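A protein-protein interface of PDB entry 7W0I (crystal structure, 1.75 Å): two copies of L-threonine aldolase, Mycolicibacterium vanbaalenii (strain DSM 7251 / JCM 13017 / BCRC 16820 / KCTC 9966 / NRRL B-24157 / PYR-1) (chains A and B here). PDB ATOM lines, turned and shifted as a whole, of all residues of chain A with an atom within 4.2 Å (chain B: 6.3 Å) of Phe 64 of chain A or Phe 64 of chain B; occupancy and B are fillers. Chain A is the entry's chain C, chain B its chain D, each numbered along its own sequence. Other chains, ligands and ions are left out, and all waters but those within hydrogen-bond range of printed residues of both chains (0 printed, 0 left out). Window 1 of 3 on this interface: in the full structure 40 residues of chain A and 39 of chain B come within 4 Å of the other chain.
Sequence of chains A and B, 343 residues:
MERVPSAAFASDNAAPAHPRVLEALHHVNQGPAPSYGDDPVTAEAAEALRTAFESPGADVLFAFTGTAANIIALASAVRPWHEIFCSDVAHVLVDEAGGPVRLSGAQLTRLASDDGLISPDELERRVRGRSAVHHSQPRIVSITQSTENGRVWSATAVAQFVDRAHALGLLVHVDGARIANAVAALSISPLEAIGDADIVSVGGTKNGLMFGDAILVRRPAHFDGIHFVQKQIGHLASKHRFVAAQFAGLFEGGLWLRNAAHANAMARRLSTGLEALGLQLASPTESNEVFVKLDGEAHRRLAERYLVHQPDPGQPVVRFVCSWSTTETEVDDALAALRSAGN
Phe 64 of chain B touches its own counterpart, Phe 64 of chain A. Phe 64 of chain A touches Thr 65 of chain B, and with the chains exchanged Thr 65 of chain A touches Phe 64 of chain B. Phe 211 of chain B touches its own counterpart, Phe 211 of chain A. His 235 of chain B touches its own counterpart, His 235 of chain A. 8 positions are printed for both chains. Of the 7 pairs that touch across the chains among the printed residues, 5 have their exchanged pair printed and touching as well.
Of the 17 printed residues of chain B, 5 touch a printed residue of chain A. Along chain B the printed residues that touch a printed residue of chain A span positions 64 to 235. Printed residues of chain A that touch a printed residue of chain B: Phe 64, Thr 65, Phe 211 and His 235. Hydrophobic or aromatic side chains of chain A that line the printed part of chain B: Phe 64, Phe 211 and His 235. Along chain A the printed residues that touch a printed residue of chain B span positions 64 to 235. Among the printed residues, no Asp or Glu carboxylate lies within 4 Å of a Lys or Arg side-chain nitrogen of the other chain.
N of Ala 68 of chain B lies within hydrogen-bond range of OG1 of Thr 65 of chain B, at 3.0 Å. The backbone carbonyl oxygen (O) of Phe 64 of chain B is in hydrogen-bond range of the backbone NH (N) of Gly 212 of chain B (3.2 Å). A ring nitrogen (ND1) of His 235 of chain A lies within hydrogen-bond range of the backbone NH (N) of Phe 64 of chain A, at 3.2 Å. O of Phe 64 of chain A is in hydrogen-bond range of N of Gly 212 of chain A (3.4 Å). A ring nitrogen (ND1) of His 235 of chain B is in hydrogen-bond range of the backbone NH (N) of Phe 64 of chain B.
Among the printed residues, pairs that only touch across the chains: Phe 211 of chain A with Phe 211 of chain B (3.1 Å), Phe 64 of chain A with Phe 64 of chain B (3.1 Å), Phe 64 of chain A with Thr 65 of chain B (3.7 Å) and Thr 65 of chain A with Phe 64 of chain B (3.8 Å).
A ring nitrogen (NE2) of His 235 of chain A sits close to the backbone carbonyl oxygen of Gly 234 of chain B (3.3 Å). OG1 of Thr 65 of chain A sits at hydrogen-bond distance from O of Gly 234 of chain B, at 2.7 Å. A ring nitrogen (NE2) of His 235 of chain B lies within hydrogen-bond range of a ring nitrogen (NE2) of His 235 of chain A, 3.1 Å away.
Of the printed residues of chain B, Phe 64 of chain A touches Phe 64 (3.1 Å) and Thr 65 (3.7 Å). Of chain A, only Phe 64 (3.1 Å) and Thr 65 (3.8 Å) come within 4 Å of Phe 64 of chain B. Of the printed residues of chain B, Thr 65 of chain A touches Phe 64 and Gly 234. Of the printed residues of chain A, Phe 211 of chain B touches Phe 211. Printed residues of chain A within 4 Å of Thr 65 of chain B: Phe 64. Of the printed residues of chain A, Gly 234 of chain B touches Thr 65 (2.7 Å) and His 235 (3.2 Å). Printed residues of chain B within 4 Å of Phe 211 of chain A: Phe 211 (3.1 Å). Phe 62 of chain B touches none of the printed residues of chain A. The nearest residue of chain B that does not touch Phe 64 of chain A is Phe 211 of chain B (4.3 Å). The nearest printed residue of chain A that does not touch Gly 234 of chain B is Phe 64 of chain A (5.0 Å).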
ATOM      1  N   ALA A  63      20.340  -5.000   7.584  1.00  0.00           N
ATOM      2  CA  ALA A  63      19.118  -4.237   7.742  1.00  0.00           C
ATOM      3  C   ALA A  63      19.050  -3.194   6.636  1.00  0.00           C
ATOM      4  O   ALA A  63      20.004  -3.000   5.873  1.00  0.00           O
ATOM      5  CB  ALA A  63      19.059  -3.568   9.116  1.00  0.00           C
ATOM      6  N   PHE A  64      17.912  -2.510   6.563  1.00  0.00           N
ATOM      7  CA  PHE A  64      17.667  -1.609   5.442  1.00  0.00           C
ATOM      8  C   PHE A  64      18.135  -0.174   5.684  1.00  0.00           C
ATOM      9  O   PHE A  64      18.337   0.557   4.705  1.00  0.00           O
ATOM     10  CB  PHE A  64      16.174  -1.605   5.099  1.00  0.00           C
ATOM     11  CG  PHE A  64      15.698  -2.848   4.378  1.00  0.00           C
ATOM     12  CD1 PHE A  64      15.049  -3.864   5.068  1.00  0.00           C
ATOM     13  CD2 PHE A  64      15.878  -2.986   3.004  1.00  0.00           C
ATOM     14  CE1 PHE A  64      14.591  -4.994   4.405  1.00  0.00           C
ATOM     15  CE2 PHE A  64      15.418  -4.114   2.330  1.00  0.00           C
ATOM     16  CZ  PHE A  64      14.775  -5.113   3.029  1.00  0.00           C
ATOM     17  N   THR A  65      18.288   0.256   6.945  1.00  0.00           N
ATOM     18  CA  THR A  65      18.738   1.612   7.280  1.00  0.00           C
ATOM     19  C   THR A  65      19.694   1.587   8.469  1.00  0.00           C
ATOM     20  O   THR A  65      19.762   0.606   9.212  1.00  0.00           O
ATOM     21  CB  THR A  65      17.576   2.547   7.639  1.00  0.00           C
ATOM     22  OG1 THR A  65      16.904   2.034   8.801  1.00  0.00           O
ATOM     23  CG2 THR A  65      16.586   2.688   6.478  1.00  0.00           C
ATOM     24  N   PHE A 211      20.641   1.073  -0.534  1.00  0.00           N
ATOM     25  CA  PHE A 211      20.111   0.934   0.809  1.00  0.00           C
ATOM     26  C   PHE A 211      20.913  -0.188   1.437  1.00  0.00           C
ATOM     27  O   PHE A 211      21.469  -1.038   0.734  1.00  0.00           O
ATOM     28  CB  PHE A 211      18.614   0.607   0.808  1.00  0.00           C
ATOM     29  CG  PHE A 211      18.314  -0.751   0.263  1.00  0.00           C
ATOM     30  CD1 PHE A 211      18.305  -1.859   1.095  1.00  0.00           C
ATOM     31  CD2 PHE A 211      18.081  -0.936  -1.079  1.00  0.00           C
ATOM     32  CE1 PHE A 211      18.054  -3.124   0.587  1.00  0.00           C
ATOM     33  CE2 PHE A 211      17.828  -2.195  -1.580  1.00  0.00           C
ATOM     34  CZ  PHE A 211      17.805  -3.288  -0.746  1.00  0.00           C
ATOM     35  N   GLY A 212      20.962  -0.199   2.755  1.00  0.00           N
ATOM     36  CA  GLY A 212      21.628  -1.303   3.405  1.00  0.00           C
ATOM     37  C   GLY A 212      22.636  -0.873   4.438  1.00  0.00           C
ATOM     38  O   GLY A 212      23.548  -0.074   4.177  1.00  0.00           O
ATOM     39  N   ASP A 213      22.467  -1.421   5.635  1.00  0.00           N
ATOM     40  CA  ASP A 213      23.379  -1.170   6.740  1.00  0.00           C
ATOM     41  C   ASP A 213      23.459  -2.445   7.564  1.00  0.00           C
ATOM     42  O   ASP A 213      22.428  -2.981   7.982  1.00  0.00           O
ATOM     43  CB  ASP A 213      22.897   0.026   7.565  1.00  0.00           C
ATOM     44  CG  ASP A 213      22.964   1.338   6.773  1.00  0.00           C
ATOM     45  OD1 ASP A 213      21.992   1.676   6.057  1.00  0.00           O
ATOM     46  OD2 ASP A 213      24.017   2.019   6.822  1.00  0.00           O
ATOM     47  N   HIS A 235      12.836  -6.040   9.235  1.00  0.00           N
ATOM     48  CA  HIS A 235      14.107  -5.825   8.558  1.00  0.00           C
ATOM     49  C   HIS A 235      14.776  -7.117   8.109  1.00  0.00           C
ATOM     50  O   HIS A 235      15.973  -7.102   7.822  1.00  0.00           O
ATOM     51  CB  HIS A 235      15.041  -4.987   9.436  1.00  0.00           C
ATOM     52  CG  HIS A 235      14.734  -3.526   9.356  1.00  0.00           C
ATOM     53  ND1 HIS A 235      15.237  -2.718   8.357  1.00  0.00           N
ATOM     54  CD2 HIS A 235      13.908  -2.747  10.093  1.00  0.00           C
ATOM     55  CE1 HIS A 235      14.744  -1.500   8.492  1.00  0.00           C
ATOM     56  NE2 HIS A 235      13.943  -1.489   9.542  1.00  0.00           N
ATOM     57  N   ALA A 237      14.814  -9.179   4.998  1.00  0.00           N
ATOM     58  CA  ALA A 237      14.363  -9.101   3.609  1.00  0.00           C
ATOM     59  C   ALA A 237      14.088 -10.488   3.049  1.00  0.00           C
ATOM     60  O   ALA A 237      14.896 -11.406   3.230  1.00  0.00           O
ATOM     61  CB  ALA A 237      15.419  -8.402   2.753  1.00  0.00           C
ATOM     62  N   PHE B  62       6.066   4.328   2.188  1.00  0.00           N
ATOM     63  CA  PHE B  62       6.778   3.202   1.593  1.00  0.00           C
ATOM     64  C   PHE B  62       7.689   2.566   2.632  1.00  0.00           C
ATOM     65  O   PHE B  62       8.499   3.258   3.258  1.00  0.00           O
ATOM     66  CB  PHE B  62       7.588   3.634   0.368  1.00  0.00           C
ATOM     67  CG  PHE B  62       6.752   4.234  -0.719  1.00  0.00           C
ATOM     68  CD1 PHE B  62       6.258   3.441  -1.750  1.00  0.00           C
ATOM     69  CD2 PHE B  62       6.435   5.586  -0.708  1.00  0.00           C
ATOM     70  CE1 PHE B  62       5.475   3.996  -2.764  1.00  0.00           C
ATOM     71  CE2 PHE B  62       5.651   6.146  -1.731  1.00  0.00           C
ATOM     72  CZ  PHE B  62       5.170   5.346  -2.746  1.00  0.00           C
ATOM     73  N   ALA B  63       7.562   1.256   2.817  1.00  0.00           N
ATOM     74  CA  ALA B  63       8.416   0.519   3.730  1.00  0.00           C
ATOM     75  C   ALA B  63       9.200  -0.508   2.926  1.00  0.00           C
ATOM     76  O   ALA B  63       8.982  -0.689   1.724  1.00  0.00           O
ATOM     77  CB  ALA B  63       7.594  -0.164   4.832  1.00  0.00           C
ATOM     78  N   PHE B  64      10.138  -1.178   3.587  1.00  0.00           N
ATOM     79  CA  PHE B  64      11.010  -2.076   2.848  1.00  0.00           C
ATOM     80  C   PHE B  64      10.463  -3.495   2.740  1.00  0.00           C
ATOM     81  O   PHE B  64      10.903  -4.233   1.851  1.00  0.00           O
ATOM     82  CB  PHE B  64      12.401  -2.115   3.491  1.00  0.00           C
ATOM     83  CG  PHE B  64      13.215  -0.852   3.299  1.00  0.00           C
ATOM     84  CD1 PHE B  64      13.257   0.129   4.281  1.00  0.00           C
ATOM     85  CD2 PHE B  64      13.952  -0.660   2.146  1.00  0.00           C
ATOM     86  CE1 PHE B  64      14.016   1.266   4.115  1.00  0.00           C
ATOM     87  CE2 PHE B  64      14.722   0.481   1.978  1.00  0.00           C
ATOM     88  CZ  PHE B  64      14.747   1.441   2.955  1.00  0.00           C
ATOM     89  N   THR B  65       9.540  -3.905   3.625  1.00  0.00           N
ATOM     90  CA  THR B  65       8.972  -5.251   3.622  1.00  0.00           C
ATOM     91  C   THR B  65       7.469  -5.213   3.905  1.00  0.00           C
ATOM     92  O   THR B  65       6.927  -4.231   4.422  1.00  0.00           O
ATOM     93  CB  THR B  65       9.637  -6.179   4.675  1.00  0.00           C
ATOM     94  OG1 THR B  65       9.328  -5.730   6.012  1.00  0.00           O
ATOM     95  CG2 THR B  65      11.157  -6.229   4.494  1.00  0.00           C
ATOM     96  N   GLY B  66       6.803  -6.328   3.591  1.00  0.00           N
ATOM     97  CA  GLY B  66       5.385  -6.451   3.907  1.00  0.00           C
ATOM     98  C   GLY B  66       5.113  -6.566   5.398  1.00  0.00           C
ATOM     99  O   GLY B  66       4.087  -6.073   5.894  1.00  0.00           O
ATOM    100  N   ALA B  68       6.872  -5.006   7.644  1.00  0.00           N
ATOM    101  CA  ALA B  68       6.951  -3.616   8.084  1.00  0.00           C
ATOM    102  C   ALA B  68       5.684  -2.845   7.733  1.00  0.00           C
ATOM    103  O   ALA B  68       5.202  -2.039   8.538  1.00  0.00           O
ATOM    104  CB  ALA B  68       8.156  -2.930   7.455  1.00  0.00           C
ATOM    105  N   ALA B  69       5.167  -3.026   6.511  1.00  0.00           N
ATOM    106  CA  ALA B  69       3.941  -2.333   6.122  1.00  0.00           C
ATOM    107  C   ALA B  69       2.801  -2.659   7.085  1.00  0.00           C
ATOM    108  O   ALA B  69       2.094  -1.753   7.565  1.00  0.00           O
ATOM    109  CB  ALA B  69       3.565  -2.700   4.682  1.00  0.00           C
ATOM    110  N   THR B 205       7.079  -6.244  -3.486  1.00  0.00           N
ATOM    111  CA  THR B 205       8.094  -7.293  -3.489  1.00  0.00           C
ATOM    112  C   THR B 205       7.616  -8.556  -4.201  1.00  0.00           C
ATOM    113  O   THR B 205       8.278  -9.057  -5.115  1.00  0.00           O
ATOM    114  CB  THR B 205       8.492  -7.631  -2.049  1.00  0.00           C
ATOM    115  OG1 THR B 205       8.860  -6.441  -1.338  1.00  0.00           O
ATOM    116  CG2 THR B 205       9.650  -8.625  -2.038  1.00  0.00           C
ATOM    117  N   PHE B 211      12.523  -4.720  -3.650  1.00  0.00           N
ATOM    118  CA  PHE B 211      12.167  -4.503  -2.258  1.00  0.00           C
ATOM    119  C   PHE B 211      11.096  -3.432  -2.233  1.00  0.00           C
ATOM    120  O   PHE B 211      10.986  -2.618  -3.156  1.00  0.00           O
ATOM    121  CB  PHE B 211      13.376  -4.058  -1.429  1.00  0.00           C
ATOM    122  CG  PHE B 211      13.976  -2.753  -1.899  1.00  0.00           C
ATOM    123  CD1 PHE B 211      13.628  -1.553  -1.292  1.00  0.00           C
ATOM    124  CD2 PHE B 211      14.852  -2.723  -2.974  1.00  0.00           C
ATOM    125  CE1 PHE B 211      14.172  -0.345  -1.736  1.00  0.00           C
ATOM    126  CE2 PHE B 211      15.400  -1.515  -3.429  1.00  0.00           C
ATOM    127  CZ  PHE B 211      15.064  -0.327  -2.800  1.00  0.00           C
ATOM    128  N   GLY B 212      10.296  -3.443  -1.176  1.00  0.00           N
ATOM    129  CA  GLY B 212       9.347  -2.335  -1.159  1.00  0.00           C
ATOM    130  C   GLY B 212       7.922  -2.823  -1.019  1.00  0.00           C
ATOM    131  O   GLY B 212       7.435  -3.678  -1.768  1.00  0.00           O
ATOM    132  N   ASP B 213       7.230  -2.256  -0.035  1.00  0.00           N
ATOM    133  CA  ASP B 213       5.815  -2.525   0.177  1.00  0.00           C
ATOM    134  C   ASP B 213       5.194  -1.248   0.726  1.00  0.00           C
ATOM    135  O   ASP B 213       5.689  -0.690   1.708  1.00  0.00           O
ATOM    136  CB  ASP B 213       5.615  -3.714   1.127  1.00  0.00           C
ATOM    137  CG  ASP B 213       6.130  -5.024   0.523  1.00  0.00           C
ATOM    138  OD1 ASP B 213       7.306  -5.371   0.772  1.00  0.00           O
ATOM    139  OD2 ASP B 213       5.377  -5.689  -0.230  1.00  0.00           O
ATOM    140  N   GLY B 234      12.858   2.240  11.697  1.00  0.00           N
ATOM    141  CA  GLY B 234      13.909   2.252  10.703  1.00  0.00           C
ATOM    142  C   GLY B 234      13.463   2.055   9.272  1.00  0.00           C
ATOM    143  O   GLY B 234      14.276   1.632   8.445  1.00  0.00           O
ATOM    144  N   HIS B 235      12.208   2.359   8.942  1.00  0.00           N
ATOM    145  CA  HIS B 235      11.685   2.128   7.599  1.00  0.00           C
ATOM    146  C   HIS B 235      11.452   3.407   6.805  1.00  0.00           C
ATOM    147  O   HIS B 235      10.773   3.359   5.770  1.00  0.00           O
ATOM    148  CB  HIS B 235      10.396   1.296   7.655  1.00  0.00           C
ATOM    149  CG  HIS B 235      10.664  -0.164   7.800  1.00  0.00           C
ATOM    150  ND1 HIS B 235      10.960  -0.983   6.730  1.00  0.00           N
ATOM    151  CD2 HIS B 235      10.757  -0.939   8.909  1.00  0.00           C
ATOM    152  CE1 HIS B 235      11.225  -2.200   7.174  1.00  0.00           C
ATOM    153  NE2 HIS B 235      11.093  -2.202   8.493  1.00  0.00           N
ATOM    154  N   LEU B 236      12.021   4.541   7.230  1.00  0.00           N
ATOM    155  CA  LEU B 236      12.040   5.755   6.405  1.00  0.00           C
ATOM    156  C   LEU B 236      13.387   5.819   5.678  1.00  0.00           C
ATOM    157  O   LEU B 236      14.414   6.171   6.272  1.00  0.00           O
ATOM    158  CB  LEU B 236      11.805   6.999   7.252  1.00  0.00           C
ATOM    159  CG  LEU B 236      11.830   8.291   6.432  1.00  0.00           C
ATOM    160  CD1 LEU B 236      10.675   8.319   5.400  1.00  0.00           C
ATOM    161  CD2 LEU B 236      11.784   9.489   7.351  1.00  0.00           C
ATOM    162  N   ALA B 237      13.375   5.480   4.385  1.00  0.00           N
ATOM    163  CA  ALA B 237      14.603   5.401   3.601  1.00  0.00           C
ATOM    164  C   ALA B 237      15.193   6.784   3.355  1.00  0.00           C
ATOM    165  O   ALA B 237      14.488   7.702   2.919  1.00  0.00           O
ATOM    166  CB  ALA B 237      14.308   4.743   2.252  1.00  0.00           C
ATOM    167  N   SER B 238      16.497   6.938   3.586  1.00  0.00           N
ATOM    168  CA  SER B 238      17.130   8.189   3.171  1.00  0.00           C
ATOM    169  C   SER B 238      17.152   8.300   1.650  1.00  0.00           C
ATOM    170  O   SER B 238      16.708   9.311   1.092  1.00  0.00           O
ATOM    171  CB  SER B 238      18.529   8.342   3.793  1.00  0.00           C
ATOM    172  OG  SER B 238      19.452   7.386   3.294  1.00  0.00           O
ATOM    173  N   VAL B 243      13.106   3.278  -3.717  1.00  0.00           N
ATOM    174  CA  VAL B 243      11.875   2.530  -3.468  1.00  0.00           C
ATOM    175  C   VAL B 243      10.736   3.126  -4.294  1.00  0.00           C
ATOM    176  O   VAL B 243       9.943   2.398  -4.933  1.00  0.00           O
ATOM    177  CB  VAL B 243      11.562   2.486  -1.953  1.00  0.00           C
ATOM    178  CG1 VAL B 243      11.333   3.866  -1.387  1.00  0.00           C
ATOM    179  CG2 VAL B 243      10.354   1.611  -1.693  1.00  0.00           C
